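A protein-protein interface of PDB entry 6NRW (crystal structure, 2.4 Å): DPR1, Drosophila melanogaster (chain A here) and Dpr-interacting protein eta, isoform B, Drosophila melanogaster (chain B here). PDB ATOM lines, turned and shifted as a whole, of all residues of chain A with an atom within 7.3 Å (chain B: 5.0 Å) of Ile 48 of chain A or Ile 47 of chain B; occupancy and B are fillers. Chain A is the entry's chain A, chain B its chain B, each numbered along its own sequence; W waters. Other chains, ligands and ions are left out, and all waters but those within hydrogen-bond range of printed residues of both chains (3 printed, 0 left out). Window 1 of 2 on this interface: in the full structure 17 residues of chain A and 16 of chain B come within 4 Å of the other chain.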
ATOM      1  N   VAL A  38     -24.114  11.708  26.280  1.00  0.00           N
ATOM      2  CA  VAL A  38     -24.996  10.892  25.456  1.00  0.00           C
ATOM      3  C   VAL A  38     -24.198   9.737  24.870  1.00  0.00           C
ATOM      4  O   VAL A  38     -23.054   9.915  24.441  1.00  0.00           O
ATOM      5  CB  VAL A  38     -25.639  11.735  24.338  1.00  0.00           C
ATOM      6  CG1 VAL A  38     -26.459  10.858  23.413  1.00  0.00           C
ATOM      7  CG2 VAL A  38     -26.483  12.847  24.936  1.00  0.00           C
ATOM      8  N   SER A  39     -24.808   8.555  24.837  1.00  0.00           N
ATOM      9  CA  SER A  39     -24.135   7.365  24.344  1.00  0.00           C
ATOM     10  C   SER A  39     -25.062   6.589  23.422  1.00  0.00           C
ATOM     11  O   SER A  39     -26.285   6.668  23.536  1.00  0.00           O
ATOM     12  CB  SER A  39     -23.686   6.459  25.493  1.00  0.00           C
ATOM     13  OG  SER A  39     -22.933   7.181  26.447  1.00  0.00           O
ATOM     14  N   TRP A  40     -24.457   5.838  22.509  1.00  0.00           N
ATOM     15  CA  TRP A  40     -25.160   4.907  21.639  1.00  0.00           C
ATOM     16  C   TRP A  40     -24.720   3.497  22.003  1.00  0.00           C
ATOM     17  O   TRP A  40     -23.520   3.243  22.142  1.00  0.00           O
ATOM     18  CB  TRP A  40     -24.861   5.176  20.163  1.00  0.00           C
ATOM     19  CG  TRP A  40     -25.670   6.269  19.541  1.00  0.00           C
ATOM     20  CD1 TRP A  40     -25.248   7.526  19.215  1.00  0.00           C
ATOM     21  CD2 TRP A  40     -27.054   6.200  19.175  1.00  0.00           C
ATOM     22  NE1 TRP A  40     -26.284   8.241  18.659  1.00  0.00           N
ATOM     23  CE2 TRP A  40     -27.404   7.449  18.629  1.00  0.00           C
ATOM     24  CE3 TRP A  40     -28.029   5.200  19.254  1.00  0.00           C
ATOM     25  CZ2 TRP A  40     -28.690   7.724  18.161  1.00  0.00           C
ATOM     26  CZ3 TRP A  40     -29.308   5.477  18.791  1.00  0.00           C
ATOM     27  CH2 TRP A  40     -29.625   6.728  18.253  1.00  0.00           C
ATOM     28  N   ILE A  41     -25.683   2.586  22.156  1.00  0.00           N
ATOM     29  CA  ILE A  41     -25.375   1.191  22.435  1.00  0.00           C
ATOM     30  C   ILE A  41     -26.199   0.303  21.518  1.00  0.00           C
ATOM     31  O   ILE A  41     -27.284   0.678  21.063  1.00  0.00           O
ATOM     32  CB  ILE A  41     -25.628   0.798  23.908  1.00  0.00           C
ATOM     33  CG1 ILE A  41     -27.107   0.964  24.262  1.00  0.00           C
ATOM     34  CG2 ILE A  41     -24.745   1.604  24.846  1.00  0.00           C
ATOM     35  CD1 ILE A  41     -27.507   0.253  25.532  1.00  0.00           C
ATOM     36  N   ARG A  42     -25.670  -0.886  21.253  1.00  0.00           N
ATOM     37  CA  ARG A  42     -26.366  -1.925  20.505  1.00  0.00           C
ATOM     38  C   ARG A  42     -27.016  -2.875  21.504  1.00  0.00           C
ATOM     39  O   ARG A  42     -26.319  -3.542  22.273  1.00  0.00           O
ATOM     40  CB  ARG A  42     -25.397  -2.664  19.586  1.00  0.00           C
ATOM     41  CG  ARG A  42     -26.053  -3.647  18.641  1.00  0.00           C
ATOM     42  CD  ARG A  42     -25.054  -4.708  18.228  1.00  0.00           C
ATOM     43  NE  ARG A  42     -24.017  -4.204  17.340  1.00  0.00           N
ATOM     44  CZ  ARG A  42     -22.773  -4.668  17.323  1.00  0.00           C
ATOM     45  NH1 ARG A  42     -22.404  -5.620  18.169  1.00  0.00           N
ATOM     46  NH2 ARG A  42     -21.887  -4.162  16.476  1.00  0.00           N
ATOM     47  N   ASP A  45     -26.435  -7.206  21.960  1.00  0.00           N
ATOM     48  CA  ASP A  45     -25.319  -7.746  22.725  1.00  0.00           C
ATOM     49  C   ASP A  45     -24.765  -6.764  23.749  1.00  0.00           C
ATOM     50  O   ASP A  45     -23.717  -7.042  24.340  1.00  0.00           O
ATOM     51  CB  ASP A  45     -24.201  -8.200  21.781  1.00  0.00           C
ATOM     52  CG  ASP A  45     -23.667  -7.070  20.923  1.00  0.00           C
ATOM     53  OD1 ASP A  45     -24.289  -5.988  20.908  1.00  0.00           O
ATOM     54  OD2 ASP A  45     -22.623  -7.264  20.264  1.00  0.00           O
ATOM     55  N   LEU A  46     -25.435  -5.630  23.977  1.00  0.00           N
ATOM     56  CA  LEU A  46     -25.005  -4.641  24.968  1.00  0.00           C
ATOM     57  C   LEU A  46     -23.627  -4.077  24.618  1.00  0.00           C
ATOM     58  O   LEU A  46     -22.801  -3.790  25.486  1.00  0.00           O
ATOM     59  CB  LEU A  46     -25.032  -5.237  26.379  1.00  0.00           C
ATOM     60  CG  LEU A  46     -24.992  -4.277  27.566  1.00  0.00           C
ATOM     61  CD1 LEU A  46     -25.860  -3.074  27.287  1.00  0.00           C
ATOM     62  CD2 LEU A  46     -25.449  -4.992  28.820  1.00  0.00           C
ATOM     63  N   HIS A  47     -23.375  -3.920  23.324  1.00  0.00           N
ATOM     64  CA  HIS A  47     -22.101  -3.410  22.839  1.00  0.00           C
ATOM     65  C   HIS A  47     -22.126  -1.888  22.839  1.00  0.00           C
ATOM     66  O   HIS A  47     -22.992  -1.277  22.206  1.00  0.00           O
ATOM     67  CB  HIS A  47     -21.807  -3.930  21.433  1.00  0.00           C
ATOM     68  CG  HIS A  47     -20.470  -3.516  20.902  1.00  0.00           C
ATOM     69  ND1 HIS A  47     -19.448  -3.076  21.716  1.00  0.00           N
ATOM     70  CD2 HIS A  47     -19.992  -3.462  19.637  1.00  0.00           C
ATOM     71  CE1 HIS A  47     -18.395  -2.777  20.975  1.00  0.00           C
ATOM     72  NE2 HIS A  47     -18.699  -3.002  19.709  1.00  0.00           N
ATOM     73  N   ILE A  48     -21.167  -1.279  23.535  1.00  0.00           N
ATOM     74  CA  ILE A  48     -21.046   0.170  23.501  1.00  0.00           C
ATOM     75  C   ILE A  48     -20.517   0.577  22.135  1.00  0.00           C
ATOM     76  O   ILE A  48     -19.553  -0.010  21.627  1.00  0.00           O
ATOM     77  CB  ILE A  48     -20.123   0.666  24.624  1.00  0.00           C
ATOM     78  CG1 ILE A  48     -20.655   0.232  25.993  1.00  0.00           C
ATOM     79  CG2 ILE A  48     -19.962   2.180  24.562  1.00  0.00           C
ATOM     80  CD1 ILE A  48     -19.747   0.633  27.152  1.00  0.00           C
ATOM     81  N   LEU A  49     -21.174   1.553  21.508  1.00  0.00           N
ATOM     82  CA  LEU A  49     -20.731   2.065  20.216  1.00  0.00           C
ATOM     83  C   LEU A  49     -19.994   3.389  20.367  1.00  0.00           C
ATOM     84  O   LEU A  49     -18.814   3.495  20.014  1.00  0.00           O
ATOM     85  CB  LEU A  49     -21.923   2.221  19.264  1.00  0.00           C
ATOM     86  CG  LEU A  49     -22.701   0.939  18.969  1.00  0.00           C
ATOM     87  CD1 LEU A  49     -23.939   1.246  18.132  1.00  0.00           C
ATOM     88  CD2 LEU A  49     -21.804  -0.076  18.284  1.00  0.00           C
ATOM     89  N   THR A  50     -20.669   4.398  20.905  1.00  0.00           N
ATOM     90  CA  THR A  50     -20.061   5.694  21.152  1.00  0.00           C
ATOM     91  C   THR A  50     -20.452   6.166  22.543  1.00  0.00           C
ATOM     92  O   THR A  50     -21.457   5.735  23.114  1.00  0.00           O
ATOM     93  CB  THR A  50     -20.480   6.749  20.111  1.00  0.00           C
ATOM     94  OG1 THR A  50     -21.860   7.089  20.292  1.00  0.00           O
ATOM     95  CG2 THR A  50     -20.264   6.244  18.691  1.00  0.00           C
ATOM     96  N   ALA A  51     -19.624   7.051  23.087  1.00  0.00           N
ATOM     97  CA  ALA A  51     -19.862   7.675  24.384  1.00  0.00           C
ATOM     98  C   ALA A  51     -19.355   9.105  24.284  1.00  0.00           C
ATOM     99  O   ALA A  51     -18.141   9.326  24.221  1.00  0.00           O
ATOM    100  CB  ALA A  51     -19.166   6.913  25.512  1.00  0.00           C
ATOM    101  N   THR A  54     -16.412  10.482  21.719  1.00  0.00           N
ATOM    102  CA  THR A  54     -15.527   9.371  21.414  1.00  0.00           C
ATOM    103  C   THR A  54     -16.293   8.142  20.944  1.00  0.00           C
ATOM    104  O   THR A  54     -17.410   7.870  21.386  1.00  0.00           O
ATOM    105  CB  THR A  54     -14.695   8.998  22.638  1.00  0.00           C
ATOM    106  OG1 THR A  54     -14.389  10.183  23.385  1.00  0.00           O
ATOM    107  CG2 THR A  54     -13.399   8.322  22.212  1.00  0.00           C
ATOM    108  N   THR A  55     -15.663   7.395  20.046  1.00  0.00           N
ATOM    109  CA  THR A  55     -16.182   6.119  19.585  1.00  0.00           C
ATOM    110  C   THR A  55     -15.539   5.029  20.429  1.00  0.00           C
ATOM    111  O   THR A  55     -14.323   5.039  20.639  1.00  0.00           O
ATOM    112  CB  THR A  55     -15.864   5.909  18.101  1.00  0.00           C
ATOM    113  OG1 THR A  55     -16.569   6.882  17.319  1.00  0.00           O
ATOM    114  CG2 THR A  55     -16.264   4.513  17.647  1.00  0.00           C
ATOM    115  N   TYR A  56     -16.353   4.104  20.934  1.00  0.00           N
ATOM    116  CA  TYR A  56     -15.804   3.013  21.730  1.00  0.00           C
ATOM    117  C   TYR A  56     -15.514   1.782  20.881  1.00  0.00           C
ATOM    118  O   TYR A  56     -14.423   1.212  20.965  1.00  0.00           O
ATOM    119  CB  TYR A  56     -16.758   2.665  22.880  1.00  0.00           C
ATOM    120  CG  TYR A  56     -16.297   1.505  23.734  1.00  0.00           C
ATOM    121  CD1 TYR A  56     -15.361   1.685  24.740  1.00  0.00           C
ATOM    122  CD2 TYR A  56     -16.813   0.232  23.541  1.00  0.00           C
ATOM    123  CE1 TYR A  56     -14.940   0.622  25.523  1.00  0.00           C
ATOM    124  CE2 TYR A  56     -16.405  -0.833  24.322  1.00  0.00           C
ATOM    125  CZ  TYR A  56     -15.466  -0.632  25.308  1.00  0.00           C
ATOM    126  OH  TYR A  56     -15.055  -1.696  26.079  1.00  0.00           O
ATOM    127  N   THR A  57     -16.471   1.376  20.047  1.00  0.00           N
ATOM    128  CA  THR A  57     -16.300   0.178  19.236  1.00  0.00           C
ATOM    129  C   THR A  57     -15.135   0.341  18.263  1.00  0.00           C
ATOM    130  O   THR A  57     -14.814   1.446  17.817  1.00  0.00           O
ATOM    131  CB  THR A  57     -17.588  -0.135  18.471  1.00  0.00           C
ATOM    132  OG1 THR A  57     -17.430  -1.354  17.735  1.00  0.00           O
ATOM    133  CG2 THR A  57     -17.932   0.993  17.506  1.00  0.00           C
ATOM    134  N   SER A  58     -14.483  -0.778  17.952  1.00  0.00           N
ATOM    135  CA  SER A  58     -13.453  -0.802  16.923  1.00  0.00           C
ATOM    136  C   SER A  58     -14.020  -1.054  15.535  1.00  0.00           C
ATOM    137  O   SER A  58     -13.269  -1.004  14.555  1.00  0.00           O
ATOM    138  CB  SER A  58     -12.396  -1.861  17.248  1.00  0.00           C
ATOM    139  OG  SER A  58     -11.687  -1.513  18.427  1.00  0.00           O
ATOM    140  N   GLU A  89     -29.892   1.987  21.082  1.00  0.00           N
ATOM    141  CA  GLU A  89     -30.382   2.832  22.165  1.00  0.00           C
ATOM    142  C   GLU A  89     -29.504   4.063  22.335  1.00  0.00           C
ATOM    143  O   GLU A  89     -28.277   3.955  22.437  1.00  0.00           O
ATOM    144  CB  GLU A  89     -30.445   2.056  23.483  1.00  0.00           C
ATOM    145  CG  GLU A  89     -30.645   2.934  24.714  1.00  0.00           C
ATOM    146  CD  GLU A  89     -30.790   2.127  25.995  1.00  0.00           C
ATOM    147  OE1 GLU A  89     -31.621   1.195  26.017  1.00  0.00           O
ATOM    148  OE2 GLU A  89     -30.092   2.436  26.985  1.00  0.00           O
ATOM    149  N   GLN A  91     -28.695   6.691  24.991  1.00  0.00           N
ATOM    150  CA  GLN A  91     -28.869   6.809  26.432  1.00  0.00           C
ATOM    151  C   GLN A  91     -28.085   7.986  26.998  1.00  0.00           C
ATOM    152  O   GLN A  91     -26.994   8.327  26.525  1.00  0.00           O
ATOM    153  CB  GLN A  91     -28.485   5.503  27.166  1.00  0.00           C
ATOM    154  CG  GLN A  91     -27.015   5.199  27.300  1.00  0.00           C
ATOM    155  CD  GLN A  91     -26.774   3.973  28.176  1.00  0.00           C
ATOM    156  OE1 GLN A  91     -25.914   3.984  29.061  1.00  0.00           O
ATOM    157  NE2 GLN A  91     -27.534   2.912  27.928  1.00  0.00           N
ATOM    158  N   ASN A  93     -26.467   9.666  30.559  1.00  0.00           N
ATOM    159  CA  ASN A  93     -25.829   9.090  31.741  1.00  0.00           C
ATOM    160  C   ASN A  93     -26.378   9.629  33.062  1.00  0.00           C
ATOM    161  O   ASN A  93     -25.648   9.704  34.057  1.00  0.00           O
ATOM    162  CB  ASN A  93     -24.310   9.277  31.662  1.00  0.00           C
ATOM    163  CG  ASN A  93     -23.891  10.728  31.671  1.00  0.00           C
ATOM    164  OD1 ASN A  93     -24.703  11.625  31.439  1.00  0.00           O
ATOM    165  ND2 ASN A  93     -22.608  10.969  31.930  1.00  0.00           N
ATOM    166  N   THR A  94     -27.655  10.014  33.084  1.00  0.00           N
ATOM    167  CA  THR A  94     -28.316  10.362  34.336  1.00  0.00           C
ATOM    168  C   THR A  94     -28.472   9.129  35.227  1.00  0.00           C
ATOM    169  O   THR A  94     -28.264   7.989  34.809  1.00  0.00           O
ATOM    170  CB  THR A  94     -29.691  10.977  34.083  1.00  0.00           C
ATOM    171  OG1 THR A  94     -30.492  10.053  33.333  1.00  0.00           O
ATOM    172  CG2 THR A  94     -29.569  12.290  33.331  1.00  0.00           C
ATOM    173  N   LYS A  97     -30.617   6.031  34.168  1.00  0.00           N
ATOM    174  CA  LYS A  97     -30.413   6.485  32.800  1.00  0.00           C
ATOM    175  C   LYS A  97     -31.717   6.984  32.182  1.00  0.00           C
ATOM    176  O   LYS A  97     -32.825   6.648  32.609  1.00  0.00           O
ATOM    177  CB  LYS A  97     -29.850   5.359  31.927  1.00  0.00           C
ATOM    178  CG  LYS A  97     -30.879   4.294  31.552  1.00  0.00           C
ATOM    179  CD  LYS A  97     -30.366   3.314  30.503  1.00  0.00           C
ATOM    180  CE  LYS A  97     -31.467   2.329  30.110  1.00  0.00           C
ATOM    181  NZ  LYS A  97     -30.984   1.215  29.229  1.00  0.00           N
ATOM    182  N   ALA B  38     -14.633  -1.658  29.639  1.00  0.00           N
ATOM    183  CA  ALA B  38     -15.822  -0.971  30.125  1.00  0.00           C
ATOM    184  C   ALA B  38     -16.639  -1.875  31.039  1.00  0.00           C
ATOM    185  O   ALA B  38     -16.702  -3.093  30.843  1.00  0.00           O
ATOM    186  CB  ALA B  38     -16.711  -0.493  28.966  1.00  0.00           C
ATOM    187  N   TRP B  39     -17.275  -1.253  32.033  1.00  0.00           N
ATOM    188  CA  TRP B  39     -18.195  -1.911  32.952  1.00  0.00           C
ATOM    189  C   TRP B  39     -19.613  -1.417  32.697  1.00  0.00           C
ATOM    190  O   TRP B  39     -19.838  -0.214  32.529  1.00  0.00           O
ATOM    191  CB  TRP B  39     -17.832  -1.628  34.413  1.00  0.00           C
ATOM    192  CG  TRP B  39     -16.817  -2.541  35.008  1.00  0.00           C
ATOM    193  CD1 TRP B  39     -15.496  -2.278  35.210  1.00  0.00           C
ATOM    194  CD2 TRP B  39     -17.045  -3.866  35.506  1.00  0.00           C
ATOM    195  NE1 TRP B  39     -14.882  -3.362  35.793  1.00  0.00           N
ATOM    196  CE2 TRP B  39     -15.811  -4.351  35.982  1.00  0.00           C
ATOM    197  CE3 TRP B  39     -18.170  -4.694  35.583  1.00  0.00           C
ATOM    198  CZ2 TRP B  39     -15.670  -5.621  36.534  1.00  0.00           C
ATOM    199  CZ3 TRP B  39     -18.031  -5.955  36.128  1.00  0.00           C
ATOM    200  CH2 TRP B  39     -16.788  -6.409  36.597  1.00  0.00           C
ATOM    201  N   LEU B  40     -20.571  -2.344  32.695  1.00  0.00           N
ATOM    202  CA  LEU B  40     -21.964  -2.007  32.455  1.00  0.00           C
ATOM    203  C   LEU B  40     -22.844  -2.763  33.435  1.00  0.00           C
ATOM    204  O   LEU B  40     -22.507  -3.864  33.876  1.00  0.00           O
ATOM    205  CB  LEU B  40     -22.434  -2.352  31.034  1.00  0.00           C
ATOM    206  CG  LEU B  40     -21.815  -1.661  29.826  1.00  0.00           C
ATOM    207  CD1 LEU B  40     -20.572  -2.420  29.375  1.00  0.00           C
ATOM    208  CD2 LEU B  40     -22.833  -1.580  28.716  1.00  0.00           C
ATOM    209  N   GLN B  45     -28.984  -2.231  31.428  1.00  0.00           N
ATOM    210  CA  GLN B  45     -28.209  -1.890  30.235  1.00  0.00           C
ATOM    211  C   GLN B  45     -27.680  -0.461  30.314  1.00  0.00           C
ATOM    212  O   GLN B  45     -27.915   0.371  29.433  1.00  0.00           O
ATOM    213  CB  GLN B  45     -29.042  -2.107  28.977  1.00  0.00           C
ATOM    214  CG  GLN B  45     -29.144  -3.563  28.568  1.00  0.00           C
ATOM    215  CD  GLN B  45     -29.844  -3.736  27.244  1.00  0.00           C
ATOM    216  OE1 GLN B  45     -31.035  -3.457  27.124  1.00  0.00           O
ATOM    217  NE2 GLN B  45     -29.113  -4.200  26.240  1.00  0.00           N
ATOM    218  N   THR B  46     -26.990  -0.170  31.410  1.00  0.00           N
ATOM    219  CA  THR B  46     -26.470   1.159  31.694  1.00  0.00           C
ATOM    220  C   THR B  46     -24.948   1.130  31.654  1.00  0.00           C
ATOM    221  O   THR B  46     -24.324   0.262  32.277  1.00  0.00           O
ATOM    222  CB  THR B  46     -26.964   1.653  33.057  1.00  0.00           C
ATOM    223  OG1 THR B  46     -28.394   1.797  33.028  1.00  0.00           O
ATOM    224  CG2 THR B  46     -26.329   2.992  33.400  1.00  0.00           C
ATOM    225  N   ILE B  47     -24.362   2.054  30.893  1.00  0.00           N
ATOM    226  CA  ILE B  47     -22.913   2.204  30.877  1.00  0.00           C
ATOM    227  C   ILE B  47     -22.464   2.783  32.209  1.00  0.00           C
ATOM    228  O   ILE B  47     -22.940   3.844  32.630  1.00  0.00           O
ATOM    229  CB  ILE B  47     -22.474   3.111  29.722  1.00  0.00           C
ATOM    230  CG1 ILE B  47     -23.034   2.605  28.398  1.00  0.00           C
ATOM    231  CG2 ILE B  47     -20.959   3.148  29.639  1.00  0.00           C
ATOM    232  CD1 ILE B  47     -22.785   3.543  27.258  1.00  0.00           C
ATOM    233  N   LEU B  48     -21.529   2.105  32.874  1.00  0.00           N
ATOM    234  CA  LEU B  48     -21.014   2.582  34.155  1.00  0.00           C
ATOM    235  C   LEU B  48     -19.642   3.243  34.022  1.00  0.00           C
ATOM    236  O   LEU B  48     -19.476   4.406  34.408  1.00  0.00           O
ATOM    237  CB  LEU B  48     -20.971   1.426  35.164  1.00  0.00           C
ATOM    238  CG  LEU B  48     -22.299   0.710  35.429  1.00  0.00           C
ATOM    239  CD1 LEU B  48     -22.112  -0.449  36.401  1.00  0.00           C
ATOM    240  CD2 LEU B  48     -23.352   1.676  35.941  1.00  0.00           C
ATOM    241  N   THR B  49     -18.649   2.527  33.480  1.00  0.00           N
ATOM    242  CA  THR B  49     -17.290   3.049  33.361  1.00  0.00           C
ATOM    243  C   THR B  49     -16.707   2.709  31.995  1.00  0.00           C
ATOM    244  O   THR B  49     -17.084   1.713  31.374  1.00  0.00           O
ATOM    245  CB  THR B  49     -16.349   2.461  34.418  1.00  0.00           C
ATOM    246  OG1 THR B  49     -16.097   1.084  34.096  1.00  0.00           O
ATOM    247  CG2 THR B  49     -16.969   2.545  35.806  1.00  0.00           C
ATOM    248  N   ILE B  50     -15.770   3.542  31.539  1.00  0.00           N
ATOM    249  CA  ILE B  50     -14.947   3.247  30.365  1.00  0.00           C
ATOM    250  C   ILE B  50     -13.505   3.635  30.677  1.00  0.00           C
ATOM    251  O   ILE B  50     -13.214   4.814  30.902  1.00  0.00           O
ATOM    252  CB  ILE B  50     -15.441   3.976  29.104  1.00  0.00           C
ATOM    253  CG1 ILE B  50     -16.848   3.493  28.732  1.00  0.00           C
ATOM    254  CG2 ILE B  50     -14.458   3.784  27.956  1.00  0.00           C
ATOM    255  CD1 ILE B  50     -17.481   4.260  27.597  1.00  0.00           C
ATOM    256  N   ILE B  55     -18.574   6.830  33.746  1.00  0.00           N
ATOM    257  CA  ILE B  55     -19.553   7.467  32.868  1.00  0.00           C
ATOM    258  C   ILE B  55     -20.830   7.805  33.624  1.00  0.00           C
ATOM    259  O   ILE B  55     -21.370   8.906  33.488  1.00  0.00           O
ATOM    260  CB  ILE B  55     -19.849   6.581  31.637  1.00  0.00           C
ATOM    261  CG1 ILE B  55     -18.831   6.829  30.520  1.00  0.00           C
ATOM    262  CG2 ILE B  55     -21.242   6.877  31.094  1.00  0.00           C
ATOM    263  CD1 ILE B  55     -17.448   6.375  30.837  1.00  0.00           C
ATOM    264  N   THR B  56     -21.329   6.873  34.432  1.00  0.00           N
ATOM    265  CA  THR B  56     -22.563   7.132  35.153  1.00  0.00           C
ATOM    266  C   THR B  56     -22.377   8.287  36.127  1.00  0.00           C
ATOM    267  O   THR B  56     -21.309   8.472  36.718  1.00  0.00           O
ATOM    268  CB  THR B  56     -23.026   5.885  35.910  1.00  0.00           C
ATOM    269  OG1 THR B  56     -24.178   6.206  36.700  1.00  0.00           O
ATOM    270  CG2 THR B  56     -21.920   5.364  36.821  1.00  0.00           C
ATOM    271  N   GLN B  89     -16.473  -5.368  29.409  1.00  0.00           N
ATOM    272  CA  GLN B  89     -16.444  -5.347  27.954  1.00  0.00           C
ATOM    273  C   GLN B  89     -15.108  -4.810  27.460  1.00  0.00           C
ATOM    274  O   GLN B  89     -14.529  -3.908  28.074  1.00  0.00           O
ATOM    275  CB  GLN B  89     -17.610  -4.494  27.434  1.00  0.00           C
ATOM    276  CG  GLN B  89     -17.757  -4.407  25.934  1.00  0.00           C
ATOM    277  CD  GLN B  89     -19.105  -3.819  25.528  1.00  0.00           C
ATOM    278  OE1 GLN B  89     -19.219  -3.136  24.508  1.00  0.00           O
ATOM    279  NE2 GLN B  89     -20.138  -4.113  26.313  1.00  0.00           N
HETATM  280  O   HOH W   1     -29.437   3.253  35.081  1.00  0.00           O
HETATM  281  O   HOH W   2     -32.728  -1.499  29.231  1.00  0.00           O
HETATM  282  O   HOH W   3     -26.316   6.225  34.856  1.00  0.00           O
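Ile 47 of chain B touches Ser 39 of chain A. Ile 41 of chain A touches Gln 45 of chain B (CD1 to O, 3.9 Å). CG2 of Ile 41 of chain A touches CD1 of Ile 47 of chain B, at 3.7 Å. Gln 45 of chain B touches Leu 46 of chain A (CG to CD1, 3.6 Å). Ala 38 of chain B touches Ile 48 of chain A (CB to CD1, 3.7 Å). Leu 40 of chain B touches Ile 48 of chain A (CD1 to CD1, 3.9 Å). CD1 of Ile 48 of chain A touches CG2 of Ile 47 of chain B, at 3.7 Å. CD1 of Ile 50 of chain B touches CB of Ala 51 of chain A (3.8 Å). Ala 38 of chain B touches Tyr 56 of chain A. CA of Thr 46 of chain B touches OE1 of Gln 91 of chain A, at 3.9 Å.
O of Ile 41 of chain A is in hydrogen-bond range of N of Glu 89 of chain A (2.9 Å). N of Arg 42 of chain A sits at hydrogen-bond distance from O of His 47 of chain A (2.9 Å). The side-chain hydroxyl of Thr 57 of chain A lies within hydrogen-bond range of a ring nitrogen (NE2) of His 47 of chain A. The backbone NH of Tyr 56 of chain A is in hydrogen-bond range of the backbone carbonyl oxygen of Leu 49 of chain A (2.7 Å). The side-chain carboxylate (OE2) of Glu 89 of chain A is in salt-bridge range of the side-chain amino group (NZ) of Lys 97 of chain A (2.7 Å). N of Ile 55 of chain B sits at hydrogen-bond distance from O of Leu 48 of chain B (2.7 Å).
Of chain B, only Ala 38 (3.7 Å), Leu 40 (3.9 Å), Ile 47 (3.7 Å) and Gln 89 (2.9 Å) come within 4 Å of Ile 48 of chain A. Ile 47 of chain B touches just these residues of chain A: Ser 39, Ile 41, Ile 48 and Gln 91. Printed residues of chain A within 4 Å of Gln 89 of chain B: Leu 46, His 47, Ile 48 and Tyr 56. Of the printed residues of chain B, His 47 of chain A touches Gln 89. Printed residues of chain A within 4 Å of Ala 38 of chain B: Ile 48 and Tyr 56. Leu 48 of chain B touches none of the printed residues of chain A. Thr 54 of chain A touches none of the printed residues of chain B.
Hydrophobic or aromatic side chains of chain B within 4 Å of the printed part of chain A: Ala 38, Leu 40, Ile 47, Ile 50 and Ile 55. Of the 22 printed residues of chain A, 11 touch a printed residue of chain B. Hydrophobic or aromatic side chains of chain A that line the printed part of chain B: Ile 41, Leu 46, His 47, Ile 48, Ala 51 and Tyr 56. Among the printed residues, no Asp or Glu carboxylate lies within 4 Å of a Lys or Arg side-chain nitrogen of the other chain.
The backbone carbonyl oxygen (O) of Leu 46 of chain A is in hydrogen-bond range of the side-chain amide nitrogen (NE2) of Gln 89 of chain B, at 2.8 Å. The side-chain amide oxygen (OE1) of Gln 89 of chain B sits at hydrogen-bond distance from a ring nitrogen (ND1) of His 47 of chain A (2.8 Å). The backbone NH (N) of Ile 48 of chain A sits at hydrogen-bond distance from the side-chain amide oxygen (OE1) of Gln 89 of chain B, 2.9 Å away. The side-chain hydroxyl (OH) of Tyr 56 of chain A is in hydrogen-bond range of the backbone carbonyl oxygen (O) of Gln 89 of chain B, 3.0 Å away. The side-chain amide nitrogen (NE2) of Gln 91 of chain A is in hydrogen-bond range of the backbone carbonyl oxygen (O) of Gln 45 of chain B (3.0 Å). The side-chain amide oxygen (OE1) of Gln 91 of chain A sits at hydrogen-bond distance from the backbone NH (N) of Ile 47 of chain B. O of Ile 55 of chain B sits at hydrogen-bond distance from ND2 of Asn 93 of chain A, 2.9 Å away. The side-chain amino group (NZ) of Lys 97 of chain A is in hydrogen-bond range of the backbone carbonyl oxygen (O) of Gln 45 of chain B, 3.2 Å away.
Water W3 lies within hydrogen-bond range of the backbone carbonyl oxygen (O) of Thr 94 of chain A (2.6 Å) and the side-chain hydroxyl (OG1) of Thr 56 of chain B (2.8 Å). Water W1 bridges the side-chain hydroxyl of Thr 46 of chain B (2.7 Å) and the backbone NH of Lys 97 of chain A (3.2 Å). Water W2 lies within hydrogen-bond range of NZ of Lys 97 of chain A (3.2 Å) and OE1 of Gln 45 of chain B (3.3 Å).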
